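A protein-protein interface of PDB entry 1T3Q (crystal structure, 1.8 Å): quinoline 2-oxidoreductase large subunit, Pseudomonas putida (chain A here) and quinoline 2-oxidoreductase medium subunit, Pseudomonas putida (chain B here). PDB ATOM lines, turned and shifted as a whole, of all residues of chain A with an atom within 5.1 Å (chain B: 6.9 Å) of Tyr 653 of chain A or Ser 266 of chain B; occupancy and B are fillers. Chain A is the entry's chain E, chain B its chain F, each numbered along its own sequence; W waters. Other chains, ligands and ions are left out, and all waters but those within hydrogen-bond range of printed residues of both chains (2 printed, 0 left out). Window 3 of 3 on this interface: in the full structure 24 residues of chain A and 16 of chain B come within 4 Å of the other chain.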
ATOM      1  N   ILE A 648      -9.331  30.201  -5.119  1.00  0.00           N
ATOM      2  CA  ILE A 648     -10.656  29.898  -4.600  1.00  0.00           C
ATOM      3  C   ILE A 648     -10.524  29.434  -3.155  1.00  0.00           C
ATOM      4  O   ILE A 648      -9.735  28.534  -2.860  1.00  0.00           O
ATOM      5  CB  ILE A 648     -11.331  28.770  -5.407  1.00  0.00           C
ATOM      6  CG1 ILE A 648     -11.511  29.203  -6.863  1.00  0.00           C
ATOM      7  CG2 ILE A 648     -12.672  28.409  -4.775  1.00  0.00           C
ATOM      8  CD1 ILE A 648     -12.089  28.116  -7.755  1.00  0.00           C
ATOM      9  N   ASP A 649     -11.285  30.052  -2.258  1.00  0.00           N
ATOM     10  CA  ASP A 649     -11.252  29.680  -0.850  1.00  0.00           C
ATOM     11  C   ASP A 649     -12.115  28.436  -0.678  1.00  0.00           C
ATOM     12  O   ASP A 649     -13.301  28.454  -0.990  1.00  0.00           O
ATOM     13  CB  ASP A 649     -11.809  30.802   0.017  1.00  0.00           C
ATOM     14  CG  ASP A 649     -11.675  30.508   1.495  1.00  0.00           C
ATOM     15  OD1 ASP A 649     -10.591  30.757   2.052  1.00  0.00           O
ATOM     16  OD2 ASP A 649     -12.647  30.009   2.094  1.00  0.00           O
ATOM     17  N   ALA A 650     -11.518  27.366  -0.169  1.00  0.00           N
ATOM     18  CA  ALA A 650     -12.223  26.103   0.021  1.00  0.00           C
ATOM     19  C   ALA A 650     -13.389  26.145   1.007  1.00  0.00           C
ATOM     20  O   ALA A 650     -14.329  25.361   0.886  1.00  0.00           O
ATOM     21  CB  ALA A 650     -11.232  25.020   0.444  1.00  0.00           C
ATOM     22  N   SER A 651     -13.334  27.052   1.974  1.00  0.00           N
ATOM     23  CA  SER A 651     -14.392  27.152   2.977  1.00  0.00           C
ATOM     24  C   SER A 651     -15.536  28.107   2.644  1.00  0.00           C
ATOM     25  O   SER A 651     -16.688  27.834   2.983  1.00  0.00           O
ATOM     26  CB  SER A 651     -13.792  27.548   4.328  1.00  0.00           C
ATOM     27  OG  SER A 651     -12.933  26.529   4.808  1.00  0.00           O
ATOM     28  N   THR A 652     -15.225  29.222   1.988  1.00  0.00           N
ATOM     29  CA  THR A 652     -16.247  30.209   1.653  1.00  0.00           C
ATOM     30  C   THR A 652     -16.554  30.300   0.162  1.00  0.00           C
ATOM     31  O   THR A 652     -17.449  31.039  -0.246  1.00  0.00           O
ATOM     32  CB  THR A 652     -15.841  31.604   2.137  1.00  0.00           C
ATOM     33  OG1 THR A 652     -14.711  32.059   1.383  1.00  0.00           O
ATOM     34  CG2 THR A 652     -15.486  31.565   3.620  1.00  0.00           C
ATOM     35  N   TYR A 653     -15.803  29.558  -0.644  1.00  0.00           N
ATOM     36  CA  TYR A 653     -15.998  29.527  -2.092  1.00  0.00           C
ATOM     37  C   TYR A 653     -15.806  30.874  -2.778  1.00  0.00           C
ATOM     38  O   TYR A 653     -16.280  31.084  -3.896  1.00  0.00           O
ATOM     39  CB  TYR A 653     -17.389  28.972  -2.411  1.00  0.00           C
ATOM     40  CG  TYR A 653     -17.737  27.782  -1.554  1.00  0.00           C
ATOM     41  CD1 TYR A 653     -18.550  27.925  -0.432  1.00  0.00           C
ATOM     42  CD2 TYR A 653     -17.197  26.527  -1.823  1.00  0.00           C
ATOM     43  CE1 TYR A 653     -18.811  26.847   0.406  1.00  0.00           C
ATOM     44  CE2 TYR A 653     -17.451  25.442  -0.992  1.00  0.00           C
ATOM     45  CZ  TYR A 653     -18.259  25.611   0.123  1.00  0.00           C
ATOM     46  OH  TYR A 653     -18.502  24.549   0.959  1.00  0.00           O
ATOM     47  N   ALA A 654     -15.107  31.785  -2.110  1.00  0.00           N
ATOM     48  CA  ALA A 654     -14.840  33.099  -2.684  1.00  0.00           C
ATOM     49  C   ALA A 654     -13.723  32.933  -3.715  1.00  0.00           C
ATOM     50  O   ALA A 654     -12.768  32.187  -3.486  1.00  0.00           O
ATOM     51  CB  ALA A 654     -14.413  34.067  -1.591  1.00  0.00           C
ATOM     52  N   THR A 655     -13.848  33.626  -4.843  1.00  0.00           N
ATOM     53  CA  THR A 655     -12.858  33.546  -5.916  1.00  0.00           C
ATOM     54  C   THR A 655     -12.173  34.879  -6.184  1.00  0.00           C
ATOM     55  O   THR A 655     -12.829  35.900  -6.378  1.00  0.00           O
ATOM     56  CB  THR A 655     -13.503  33.089  -7.237  1.00  0.00           C
ATOM     57  OG1 THR A 655     -14.120  31.814  -7.049  1.00  0.00           O
ATOM     58  CG2 THR A 655     -12.453  32.985  -8.334  1.00  0.00           C
ATOM     59  N   PRO A 775     -20.147  31.757  -6.135  1.00  0.00           N
ATOM     60  CA  PRO A 775     -19.871  30.895  -4.985  1.00  0.00           C
ATOM     61  C   PRO A 775     -20.881  29.749  -4.919  1.00  0.00           C
ATOM     62  O   PRO A 775     -20.534  28.629  -4.554  1.00  0.00           O
ATOM     63  CB  PRO A 775     -19.947  31.855  -3.783  1.00  0.00           C
ATOM     64  CG  PRO A 775     -20.552  33.125  -4.328  1.00  0.00           C
ATOM     65  CD  PRO A 775     -20.101  33.178  -5.758  1.00  0.00           C
ATOM     66  N   ILE A 778     -19.730  27.153  -7.346  1.00  0.00           N
ATOM     67  CA  ILE A 778     -18.527  26.474  -6.876  1.00  0.00           C
ATOM     68  C   ILE A 778     -18.920  25.523  -5.744  1.00  0.00           C
ATOM     69  O   ILE A 778     -18.511  24.358  -5.719  1.00  0.00           O
ATOM     70  CB  ILE A 778     -17.479  27.474  -6.352  1.00  0.00           C
ATOM     71  CG1 ILE A 778     -16.951  28.322  -7.512  1.00  0.00           C
ATOM     72  CG2 ILE A 778     -16.344  26.722  -5.673  1.00  0.00           C
ATOM     73  CD1 ILE A 778     -15.990  29.413  -7.092  1.00  0.00           C
ATOM     74  N   PHE A 779     -19.718  26.030  -4.810  1.00  0.00           N
ATOM     75  CA  PHE A 779     -20.192  25.241  -3.677  1.00  0.00           C
ATOM     76  C   PHE A 779     -20.832  23.949  -4.178  1.00  0.00           C
ATOM     77  O   PHE A 779     -20.498  22.856  -3.721  1.00  0.00           O
ATOM     78  CB  PHE A 779     -21.215  26.061  -2.879  1.00  0.00           C
ATOM     79  CG  PHE A 779     -22.042  25.248  -1.922  1.00  0.00           C
ATOM     80  CD1 PHE A 779     -21.477  24.700  -0.778  1.00  0.00           C
ATOM     81  CD2 PHE A 779     -23.397  25.043  -2.166  1.00  0.00           C
ATOM     82  CE1 PHE A 779     -22.247  23.960   0.116  1.00  0.00           C
ATOM     83  CE2 PHE A 779     -24.180  24.302  -1.279  1.00  0.00           C
ATOM     84  CZ  PHE A 779     -23.603  23.760  -0.135  1.00  0.00           C
ATOM     85  N   ILE A 782     -18.394  21.371  -5.957  1.00  0.00           N
ATOM     86  CA  ILE A 782     -17.591  20.642  -4.981  1.00  0.00           C
ATOM     87  C   ILE A 782     -18.447  19.651  -4.199  1.00  0.00           C
ATOM     88  O   ILE A 782     -18.042  18.513  -3.966  1.00  0.00           O
ATOM     89  CB  ILE A 782     -16.909  21.602  -3.987  1.00  0.00           C
ATOM     90  CG1 ILE A 782     -15.837  22.420  -4.710  1.00  0.00           C
ATOM     91  CG2 ILE A 782     -16.306  20.813  -2.831  1.00  0.00           C
ATOM     92  CD1 ILE A 782     -15.104  23.401  -3.818  1.00  0.00           C
ATOM     93  N   TYR B 183     -19.833  37.666   5.451  1.00  0.00           N
ATOM     94  CA  TYR B 183     -19.492  37.235   4.105  1.00  0.00           C
ATOM     95  C   TYR B 183     -20.289  38.104   3.140  1.00  0.00           C
ATOM     96  O   TYR B 183     -21.518  38.136   3.200  1.00  0.00           O
ATOM     97  CB  TYR B 183     -19.879  35.769   3.895  1.00  0.00           C
ATOM     98  CG  TYR B 183     -19.488  35.220   2.540  1.00  0.00           C
ATOM     99  CD1 TYR B 183     -18.219  34.684   2.322  1.00  0.00           C
ATOM    100  CD2 TYR B 183     -20.385  35.243   1.472  1.00  0.00           C
ATOM    101  CE1 TYR B 183     -17.853  34.178   1.074  1.00  0.00           C
ATOM    102  CE2 TYR B 183     -20.028  34.739   0.217  1.00  0.00           C
ATOM    103  CZ  TYR B 183     -18.760  34.206   0.029  1.00  0.00           C
ATOM    104  OH  TYR B 183     -18.401  33.694  -1.200  1.00  0.00           O
ATOM    105  N   ARG B 185     -20.238  39.481  -1.159  1.00  0.00           N
ATOM    106  CA  ARG B 185     -19.639  39.308  -2.485  1.00  0.00           C
ATOM    107  C   ARG B 185     -18.326  40.092  -2.622  1.00  0.00           C
ATOM    108  O   ARG B 185     -17.327  39.572  -3.127  1.00  0.00           O
ATOM    109  CB  ARG B 185     -20.646  39.717  -3.563  1.00  0.00           C
ATOM    110  CG  ARG B 185     -21.833  38.748  -3.679  1.00  0.00           C
ATOM    111  CD  ARG B 185     -21.695  37.831  -4.894  1.00  0.00           C
ATOM    112  NE  ARG B 185     -20.332  37.333  -5.051  1.00  0.00           N
ATOM    113  CZ  ARG B 185     -19.882  36.696  -6.127  1.00  0.00           C
ATOM    114  NH1 ARG B 185     -20.682  36.464  -7.160  1.00  0.00           N
ATOM    115  NH2 ARG B 185     -18.616  36.307  -6.174  1.00  0.00           N
ATOM    116  N   VAL B 193     -24.364  36.664   5.162  1.00  0.00           N
ATOM    117  CA  VAL B 193     -24.421  36.234   6.551  1.00  0.00           C
ATOM    118  C   VAL B 193     -23.404  37.041   7.344  1.00  0.00           C
ATOM    119  O   VAL B 193     -22.364  37.433   6.814  1.00  0.00           O
ATOM    120  CB  VAL B 193     -24.071  34.726   6.721  1.00  0.00           C
ATOM    121  CG1 VAL B 193     -25.005  33.868   5.889  1.00  0.00           C
ATOM    122  CG2 VAL B 193     -22.623  34.469   6.325  1.00  0.00           C
ATOM    123  N   THR B 248     -25.810  27.405  13.973  1.00  0.00           N
ATOM    124  CA  THR B 248     -26.536  27.451  12.707  1.00  0.00           C
ATOM    125  C   THR B 248     -27.637  26.407  12.552  1.00  0.00           C
ATOM    126  O   THR B 248     -28.473  26.516  11.656  1.00  0.00           O
ATOM    127  CB  THR B 248     -25.568  27.313  11.514  1.00  0.00           C
ATOM    128  OG1 THR B 248     -24.868  26.068  11.607  1.00  0.00           O
ATOM    129  CG2 THR B 248     -24.558  28.455  11.510  1.00  0.00           C
ATOM    130  N   ARG B 261     -30.159  28.158   0.052  1.00  0.00           N
ATOM    131  CA  ARG B 261     -30.272  27.954   1.489  1.00  0.00           C
ATOM    132  C   ARG B 261     -29.025  27.227   2.009  1.00  0.00           C
ATOM    133  O   ARG B 261     -28.438  27.625   3.017  1.00  0.00           O
ATOM    134  CB  ARG B 261     -31.521  27.122   1.795  1.00  0.00           C
ATOM    135  CG  ARG B 261     -31.532  26.493   3.177  1.00  0.00           C
ATOM    136  N   ASP B 262     -28.626  26.167   1.308  1.00  0.00           N
ATOM    137  CA  ASP B 262     -27.461  25.376   1.697  1.00  0.00           C
ATOM    138  C   ASP B 262     -26.173  26.195   1.718  1.00  0.00           C
ATOM    139  O   ASP B 262     -25.375  26.080   2.648  1.00  0.00           O
ATOM    140  CB  ASP B 262     -27.298  24.181   0.753  1.00  0.00           C
ATOM    141  CG  ASP B 262     -28.383  23.135   0.944  1.00  0.00           C
ATOM    142  OD2 ASP B 262     -29.203  23.298   1.874  1.00  0.00           O
ATOM    143  N   LEU B 263     -25.965  27.009   0.687  1.00  0.00           N
ATOM    144  CA  LEU B 263     -24.770  27.841   0.624  1.00  0.00           C
ATOM    145  C   LEU B 263     -24.738  28.764   1.836  1.00  0.00           C
ATOM    146  O   LEU B 263     -23.701  28.919   2.482  1.00  0.00           O
ATOM    147  CB  LEU B 263     -24.764  28.684  -0.654  1.00  0.00           C
ATOM    148  CG  LEU B 263     -23.651  29.734  -0.720  1.00  0.00           C
ATOM    149  CD1 LEU B 263     -22.292  29.057  -0.699  1.00  0.00           C
ATOM    150  CD2 LEU B 263     -23.821  30.570  -1.977  1.00  0.00           C
ATOM    151  N   ARG B 264     -25.888  29.369   2.129  1.00  0.00           N
ATOM    152  CA  ARG B 264     -26.059  30.290   3.253  1.00  0.00           C
ATOM    153  C   ARG B 264     -25.652  29.641   4.568  1.00  0.00           C
ATOM    154  O   ARG B 264     -24.918  30.225   5.369  1.00  0.00           O
ATOM    155  CB  ARG B 264     -27.522  30.712   3.362  1.00  0.00           C
ATOM    156  CG  ARG B 264     -28.123  31.251   2.085  1.00  0.00           C
ATOM    157  CD  ARG B 264     -27.932  32.725   1.995  1.00  0.00           C
ATOM    158  NE  ARG B 264     -28.576  33.317   0.828  1.00  0.00           N
ATOM    159  CZ  ARG B 264     -28.664  34.627   0.645  1.00  0.00           C
ATOM    160  NH1 ARG B 264     -28.158  35.444   1.556  1.00  0.00           N
ATOM    161  NH2 ARG B 264     -29.223  35.123  -0.447  1.00  0.00           N
ATOM    162  N   LEU B 265     -26.159  28.438   4.799  1.00  0.00           N
ATOM    163  CA  LEU B 265     -25.851  27.706   6.015  1.00  0.00           C
ATOM    164  C   LEU B 265     -24.370  27.367   6.088  1.00  0.00           C
ATOM    165  O   LEU B 265     -23.746  27.498   7.141  1.00  0.00           O
ATOM    166  CB  LEU B 265     -26.684  26.428   6.078  1.00  0.00           C
ATOM    167  CG  LEU B 265     -28.166  26.694   6.338  1.00  0.00           C
ATOM    168  CD1 LEU B 265     -28.964  25.401   6.229  1.00  0.00           C
ATOM    169  CD2 LEU B 265     -28.318  27.321   7.722  1.00  0.00           C
ATOM    170  N   SER B 266     -23.812  26.936   4.962  1.00  0.00           N
ATOM    171  CA  SER B 266     -22.400  26.587   4.899  1.00  0.00           C
ATOM    172  C   SER B 266     -21.569  27.815   5.254  1.00  0.00           C
ATOM    173  O   SER B 266     -20.630  27.733   6.052  1.00  0.00           O
ATOM    174  CB  SER B 266     -22.045  26.092   3.490  1.00  0.00           C
ATOM    175  OG  SER B 266     -20.712  25.621   3.430  1.00  0.00           O
ATOM    176  N   LEU B 267     -21.933  28.954   4.669  1.00  0.00           N
ATOM    177  CA  LEU B 267     -21.230  30.205   4.917  1.00  0.00           C
ATOM    178  C   LEU B 267     -21.418  30.671   6.362  1.00  0.00           C
ATOM    179  O   LEU B 267     -20.478  31.155   6.998  1.00  0.00           O
ATOM    180  CB  LEU B 267     -21.727  31.289   3.957  1.00  0.00           C
ATOM    181  CG  LEU B 267     -21.417  31.099   2.467  1.00  0.00           C
ATOM    182  CD1 LEU B 267     -22.100  32.198   1.666  1.00  0.00           C
ATOM    183  CD2 LEU B 267     -19.907  31.136   2.240  1.00  0.00           C
ATOM    184  N   ALA B 268     -22.638  30.529   6.870  1.00  0.00           N
ATOM    185  CA  ALA B 268     -22.953  30.931   8.234  1.00  0.00           C
ATOM    186  C   ALA B 268     -22.060  30.183   9.216  1.00  0.00           C
ATOM    187  O   ALA B 268     -21.518  30.769  10.160  1.00  0.00           O
ATOM    188  CB  ALA B 268     -24.421  30.644   8.532  1.00  0.00           C
ATOM    189  N   LYS B 269     -21.910  28.886   8.983  1.00  0.00           N
ATOM    190  CA  LYS B 269     -21.086  28.032   9.825  1.00  0.00           C
ATOM    191  C   LYS B 269     -19.616  28.471   9.759  1.00  0.00           C
ATOM    192  O   LYS B 269     -18.965  28.650  10.791  1.00  0.00           O
ATOM    193  CB  LYS B 269     -21.248  26.579   9.363  1.00  0.00           C
ATOM    194  CG  LYS B 269     -20.755  25.512  10.328  1.00  0.00           C
ATOM    195  N   ALA B 270     -19.104  28.665   8.547  1.00  0.00           N
ATOM    196  CA  ALA B 270     -17.713  29.076   8.353  1.00  0.00           C
ATOM    197  C   ALA B 270     -17.393  30.417   9.002  1.00  0.00           C
ATOM    198  O   ALA B 270     -16.365  30.564   9.674  1.00  0.00           O
ATOM    199  CB  ALA B 270     -17.386  29.134   6.859  1.00  0.00           C
ATOM    200  N   ILE B 271     -18.265  31.400   8.791  1.00  0.00           N
ATOM    201  CA  ILE B 271     -18.066  32.728   9.358  1.00  0.00           C
ATOM    202  C   ILE B 271     -18.142  32.696  10.887  1.00  0.00           C
ATOM    203  O   ILE B 271     -17.328  33.327  11.571  1.00  0.00           O
ATOM    204  CB  ILE B 271     -19.125  33.730   8.829  1.00  0.00           C
ATOM    205  CG1 ILE B 271     -19.006  33.864   7.307  1.00  0.00           C
ATOM    206  CG2 ILE B 271     -18.930  35.092   9.482  1.00  0.00           C
ATOM    207  CD1 ILE B 271     -17.685  34.422   6.835  1.00  0.00           C
HETATM  208  O   HOH W   1     -17.841  25.538   3.936  1.00  0.00           O
HETATM  209  O   HOH W   2     -16.097  35.294  -4.946  1.00  0.00           O
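The side-chain hydroxyl of Tyr 653 of chain A lies within hydrogen-bond range of the side-chain hydroxyl of Ser 266 of chain B (3.5 Å). OH of Tyr 183 of chain B sits at hydrogen-bond distance from O of Thr 652 of chain A (3.0 Å).
The backbone NH (N) of Asp 649 of chain A is in hydrogen-bond range of the backbone carbonyl oxygen (O) of Ala 654 of chain A. The side-chain carboxylate (OD2) of Asp 649 of chain A lies within hydrogen-bond range of the backbone NH (N) of Thr 652 of chain A (2.7 Å). O of Val 193 of chain B is in hydrogen-bond range of N of Tyr 183 of chain B (2.9 Å).
Among the printed residues, merely in contact across the chains: Pro 775 of chain A with Arg 185 of chain B, Thr 652 of chain A with Leu 267 of chain B, Pro 775 of chain A with Tyr 183 of chain B, Phe 779 of chain A with Asp 262 of chain B, Phe 779 of chain A with Leu 263 of chain B, Ala 654 of chain A with Tyr 183 of chain B, Tyr 653 of chain A with Leu 263 of chain B and Phe 779 of chain A with Ser 266 of chain B.
Tyr 653 of chain A touches two residues of chain B. Of the printed residues of chain A, Ser 266 of chain B touches Tyr 653 (3.5 Å) and Phe 779 (3.996 Å). Of the printed residues of chain B, Pro 775 of chain A touches Tyr 183 (3.5 Å) and Arg 185 (3.5 Å). Of the printed residues of chain A, Tyr 183 of chain B touches Thr 652, Ala 654 and Pro 775. Of the printed residues of chain A, Leu 267 of chain B touches Thr 652. Printed residues of chain A within 4 Å of Leu 263 of chain B: Tyr 653 (3.9 Å) and Phe 779 (3.8 Å). Arg 261 of chain B touches none of the printed residues of chain A. Ile 648 of chain A touches none of the printed residues of chain B. The nearest printed residue of chain A that does not touch Ser 266 of chain B is Ser 651 of chain A (4.6 Å).
Of the 15 printed residues of chain B, 6 touch a printed residue of chain A. Hydrophobic or aromatic side chains of chain B within 4 Å of the printed part of chain A: Tyr 183, Leu 263 and Leu 267. Of the 12 printed residues of chain A, 5 touch a printed residue of chain B. Printed residues of chain A that touch a printed residue of chain B: Thr 652, Tyr 653, Ala 654, Pro 775 and Phe 779. Among the printed residues, 10 pairs touch across the chains.
Water W1 lies within hydrogen-bond range of the backbone carbonyl oxygen of Ser 651 of chain A (2.7 Å), the side-chain hydroxyl of Ser 266 of chain B (2.9 Å) and the side-chain hydroxyl of Tyr 653 of chain A (3.2 Å). Water W2 bridges N of Thr 655 of chain A and NH2 of Arg 185 of chain B.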
